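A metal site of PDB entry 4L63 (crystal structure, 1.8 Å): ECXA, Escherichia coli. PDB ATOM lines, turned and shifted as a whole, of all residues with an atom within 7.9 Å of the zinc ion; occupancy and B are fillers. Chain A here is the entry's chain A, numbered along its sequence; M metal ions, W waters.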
ATOM      1  N   GLY A 104      22.202  14.433  32.429  1.00  0.00           N
ATOM      2  CA  GLY A 104      22.742  15.312  33.450  1.00  0.00           C
ATOM      3  C   GLY A 104      22.479  16.779  33.174  1.00  0.00           C
ATOM      4  O   GLY A 104      22.077  17.156  32.068  1.00  0.00           O
ATOM      5  N   SER A 105      22.709  17.609  34.180  1.00  0.00           N
ATOM      6  CA  SER A 105      22.426  19.036  34.096  1.00  0.00           C
ATOM      7  C   SER A 105      23.145  19.817  35.207  1.00  0.00           C
ATOM      8  O   SER A 105      23.203  19.374  36.357  1.00  0.00           O
ATOM      9  CB  SER A 105      20.908  19.275  34.174  1.00  0.00           C
ATOM     10  OG  SER A 105      20.587  20.649  34.087  1.00  0.00           O
ATOM     11  N   THR A 106      23.678  20.992  34.865  1.00  0.00           N
ATOM     12  CA  THR A 106      24.394  21.818  35.840  1.00  0.00           C
ATOM     13  C   THR A 106      24.007  23.291  35.732  1.00  0.00           C
ATOM     14  O   THR A 106      23.927  23.848  34.637  1.00  0.00           O
ATOM     15  CB  THR A 106      25.934  21.693  35.660  1.00  0.00           C
ATOM     16  OG1 THR A 106      26.344  20.375  36.012  1.00  0.00           O
ATOM     17  CG2 THR A 106      26.671  22.707  36.534  1.00  0.00           C
ATOM     18  N   THR A 157      29.149  11.475  32.124  1.00  0.00           N
ATOM     19  CA  THR A 157      28.140  12.473  32.467  1.00  0.00           C
ATOM     20  C   THR A 157      28.575  13.344  33.641  1.00  0.00           C
ATOM     21  O   THR A 157      28.450  14.565  33.586  1.00  0.00           O
ATOM     22  CB  THR A 157      26.783  11.811  32.814  1.00  0.00           C
ATOM     23  OG1 THR A 157      26.313  11.056  31.689  1.00  0.00           O
ATOM     24  CG2 THR A 157      25.760  12.864  33.182  1.00  0.00           C
ATOM     25  N   HIS A 160      31.697  15.454  32.674  1.00  0.00           N
ATOM     26  CA  HIS A 160      31.192  16.525  31.813  1.00  0.00           C
ATOM     27  C   HIS A 160      30.538  17.632  32.637  1.00  0.00           C
ATOM     28  O   HIS A 160      30.808  18.820  32.431  1.00  0.00           O
ATOM     29  CB  HIS A 160      30.203  15.943  30.791  1.00  0.00           C
ATOM     30  CG  HIS A 160      29.538  16.961  29.920  1.00  0.00           C
ATOM     31  ND1 HIS A 160      30.072  17.373  28.712  1.00  0.00           N
ATOM     32  CD2 HIS A 160      28.376  17.645  30.080  1.00  0.00           C
ATOM     33  CE1 HIS A 160      29.255  18.270  28.163  1.00  0.00           C
ATOM     34  NE2 HIS A 160      28.224  18.446  28.976  1.00  0.00           N
ATOM     35  N   GLU A 161      29.699  17.258  33.596  1.00  0.00           N
ATOM     36  CA  GLU A 161      29.030  18.246  34.438  1.00  0.00           C
ATOM     37  C   GLU A 161      30.022  19.000  35.338  1.00  0.00           C
ATOM     38  O   GLU A 161      29.839  20.192  35.604  1.00  0.00           O
ATOM     39  CB  GLU A 161      27.925  17.585  35.282  1.00  0.00           C
ATOM     40  CG  GLU A 161      26.756  17.022  34.463  1.00  0.00           C
ATOM     41  CD  GLU A 161      26.219  17.986  33.406  1.00  0.00           C
ATOM     42  OE1 GLU A 161      25.970  19.164  33.741  1.00  0.00           O
ATOM     43  OE2 GLU A 161      26.043  17.558  32.241  1.00  0.00           O
ATOM     44  N   GLY A 163      32.953  19.822  34.394  1.00  0.00           N
ATOM     45  CA  GLY A 163      33.447  20.842  33.484  1.00  0.00           C
ATOM     46  C   GLY A 163      32.627  22.119  33.592  1.00  0.00           C
ATOM     47  O   GLY A 163      33.183  23.219  33.641  1.00  0.00           O
ATOM     48  N   HIS A 164      31.298  21.962  33.655  1.00  0.00           N
ATOM     49  CA  HIS A 164      30.379  23.085  33.783  1.00  0.00           C
ATOM     50  C   HIS A 164      30.534  23.780  35.140  1.00  0.00           C
ATOM     51  O   HIS A 164      30.504  25.011  35.224  1.00  0.00           O
ATOM     52  CB  HIS A 164      28.940  22.601  33.601  1.00  0.00           C
ATOM     53  CG  HIS A 164      28.587  22.277  32.185  1.00  0.00           C
ATOM     54  ND1 HIS A 164      28.992  23.058  31.120  1.00  0.00           N
ATOM     55  CD2 HIS A 164      27.866  21.265  31.657  1.00  0.00           C
ATOM     56  CE1 HIS A 164      28.530  22.542  29.997  1.00  0.00           C
ATOM     57  NE2 HIS A 164      27.853  21.444  30.293  1.00  0.00           N
ATOM     58  N   LEU A 168      33.305  25.874  32.318  1.00  0.00           N
ATOM     59  CA  LEU A 168      33.338  25.575  30.889  1.00  0.00           C
ATOM     60  C   LEU A 168      31.937  25.405  30.319  1.00  0.00           C
ATOM     61  O   LEU A 168      30.992  25.026  31.025  1.00  0.00           O
ATOM     62  CB  LEU A 168      34.161  24.318  30.621  1.00  0.00           C
ATOM     63  CG  LEU A 168      35.618  24.402  31.057  1.00  0.00           C
ATOM     64  CD1 LEU A 168      36.390  23.165  30.630  1.00  0.00           C
ATOM     65  CD2 LEU A 168      36.280  25.670  30.522  1.00  0.00           C
ATOM     66  N   LEU A 169      31.802  25.705  29.035  1.00  0.00           N
ATOM     67  CA  LEU A 169      30.546  25.486  28.318  1.00  0.00           C
ATOM     68  C   LEU A 169      30.806  24.407  27.271  1.00  0.00           C
ATOM     69  O   LEU A 169      31.747  23.637  27.412  1.00  0.00           O
ATOM     70  CB  LEU A 169      30.051  26.800  27.701  1.00  0.00           C
ATOM     71  CG  LEU A 169      29.760  27.893  28.737  1.00  0.00           C
ATOM     72  CD1 LEU A 169      29.596  29.252  28.077  1.00  0.00           C
ATOM     73  CD2 LEU A 169      28.519  27.564  29.562  1.00  0.00           C
ATOM     74  N   HIS A 170      29.978  24.343  26.232  1.00  0.00           N
ATOM     75  CA  HIS A 170      30.184  23.350  25.189  1.00  0.00           C
ATOM     76  C   HIS A 170      31.073  23.863  24.067  1.00  0.00           C
ATOM     77  O   HIS A 170      31.140  25.065  23.835  1.00  0.00           O
ATOM     78  CB  HIS A 170      28.849  22.903  24.586  1.00  0.00           C
ATOM     79  CG  HIS A 170      27.957  22.224  25.568  1.00  0.00           C
ATOM     80  ND1 HIS A 170      26.608  22.470  25.629  1.00  0.00           N
ATOM     81  CD2 HIS A 170      28.218  21.299  26.520  1.00  0.00           C
ATOM     82  CE1 HIS A 170      26.072  21.734  26.594  1.00  0.00           C
ATOM     83  NE2 HIS A 170      27.030  21.010  27.143  1.00  0.00           N
ATOM     84  N   GLU A 173      29.727  26.616  21.591  1.00  0.00           N
ATOM     85  CA  GLU A 173      28.921  27.696  22.152  1.00  0.00           C
ATOM     86  C   GLU A 173      29.654  29.026  22.259  1.00  0.00           C
ATOM     87  O   GLU A 173      29.198  29.940  22.967  1.00  0.00           O
ATOM     88  CB  GLU A 173      28.359  27.268  23.511  1.00  0.00           C
ATOM     89  CG  GLU A 173      27.176  26.304  23.361  1.00  0.00           C
ATOM     90  CD  GLU A 173      26.763  25.642  24.652  1.00  0.00           C
ATOM     91  OE1 GLU A 173      27.481  25.774  25.669  1.00  0.00           O
ATOM     92  OE2 GLU A 173      25.693  24.983  24.645  1.00  0.00           O
ATOM     93  N   ILE A 198      35.881  16.573  26.438  1.00  0.00           N
ATOM     94  CA  ILE A 198      34.779  15.907  27.107  1.00  0.00           C
ATOM     95  C   ILE A 198      33.612  16.894  27.252  1.00  0.00           C
ATOM     96  O   ILE A 198      32.526  16.537  27.730  1.00  0.00           O
ATOM     97  CB  ILE A 198      35.217  15.338  28.467  1.00  0.00           C
ATOM     98  CG1 ILE A 198      34.206  14.301  28.988  1.00  0.00           C
ATOM     99  CG2 ILE A 198      35.503  16.477  29.463  1.00  0.00           C
ATOM    100  CD1 ILE A 198      34.729  13.433  30.111  1.00  0.00           C
ATOM    101  N   MET A 199      33.826  18.139  26.814  1.00  0.00           N
ATOM    102  CA  MET A 199      32.765  19.150  26.831  1.00  0.00           C
ATOM    103  C   MET A 199      32.135  19.335  25.456  1.00  0.00           C
ATOM    104  O   MET A 199      31.513  20.380  25.200  1.00  0.00           O
ATOM    105  CB  MET A 199      33.300  20.495  27.331  1.00  0.00           C
ATOM    106  CG  MET A 199      33.999  20.404  28.674  1.00  0.00           C
ATOM    107  SD  MET A 199      32.907  19.701  29.931  1.00  0.00           S
ATOM    108  CE  MET A 199      31.599  20.937  30.007  1.00  0.00           C
ATOM    109  N   LEU A 200      32.305  18.360  24.578  1.00  0.00           N
ATOM    110  CA  LEU A 200      31.562  18.320  23.325  1.00  0.00           C
ATOM    111  C   LEU A 200      30.076  18.495  23.612  1.00  0.00           C
ATOM    112  O   LEU A 200      29.567  17.963  24.591  1.00  0.00           O
ATOM    113  CB  LEU A 200      31.795  17.010  22.577  1.00  0.00           C
ATOM    114  CG  LEU A 200      33.178  16.810  21.958  1.00  0.00           C
ATOM    115  CD1 LEU A 200      33.215  15.482  21.192  1.00  0.00           C
ATOM    116  CD2 LEU A 200      33.552  17.981  21.058  1.00  0.00           C
ATOM    117  N   ASN A 201      29.390  19.254  22.764  1.00  0.00           N
ATOM    118  CA  ASN A 201      27.952  19.408  22.893  1.00  0.00           C
ATOM    119  C   ASN A 201      27.271  18.077  22.566  1.00  0.00           C
ATOM    120  O   ASN A 201      27.395  17.560  21.453  1.00  0.00           O
ATOM    121  CB  ASN A 201      27.450  20.522  21.963  1.00  0.00           C
ATOM    122  CG  ASN A 201      26.050  20.986  22.315  1.00  0.00           C
ATOM    123  OD1 ASN A 201      25.204  20.186  22.704  1.00  0.00           O
ATOM    124  ND2 ASN A 201      25.801  22.281  22.156  1.00  0.00           N
ATOM    125  N   GLY A 202      26.567  17.520  23.559  1.00  0.00           N
ATOM    126  CA  GLY A 202      25.973  16.201  23.435  1.00  0.00           C
ATOM    127  C   GLY A 202      24.814  16.158  22.471  1.00  0.00           C
ATOM    128  O   GLY A 202      24.369  15.082  22.056  1.00  0.00           O
ATOM    129  N   SER A 203      24.294  17.336  22.115  1.00  0.00           N
ATOM    130  CA  SER A 203      23.243  17.440  21.123  1.00  0.00           C
ATOM    131  C   SER A 203      23.793  17.202  19.718  1.00  0.00           C
ATOM    132  O   SER A 203      23.052  16.869  18.798  1.00  0.00           O
ATOM    133  CB  SER A 203      22.566  18.813  21.186  1.00  0.00           C
ATOM    134  OG  SER A 203      21.874  19.004  22.414  1.00  0.00           O
HETATM  135 ZN    ZN M   1      26.817  20.033  28.964  1.00  0.00          ZN
HETATM  136  O   HOH W   1      24.980  19.129  30.385  1.00  0.00           O
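The zinc ion is bound by NE2 of His 170 (2.1 Å), NE2 of His 160 (2.1 Å), NE2 of His 164 (2.2 Å) and water W1 (2.5 Å).
A ring nitrogen (ND1) of His 170 is in hydrogen-bond range of the side-chain carboxylate (OE2) of Glu 173 (2.8 Å).
ND1 of His 164 is in hydrogen-bond range of O of Leu 168 (2.8 Å).
ND1 of His 160 lies within hydrogen-bond range of O of Ile 198 (2.8 Å).
Three residues have an atom within 4 Å of the zinc ion: His 160, His 164 and His 170.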
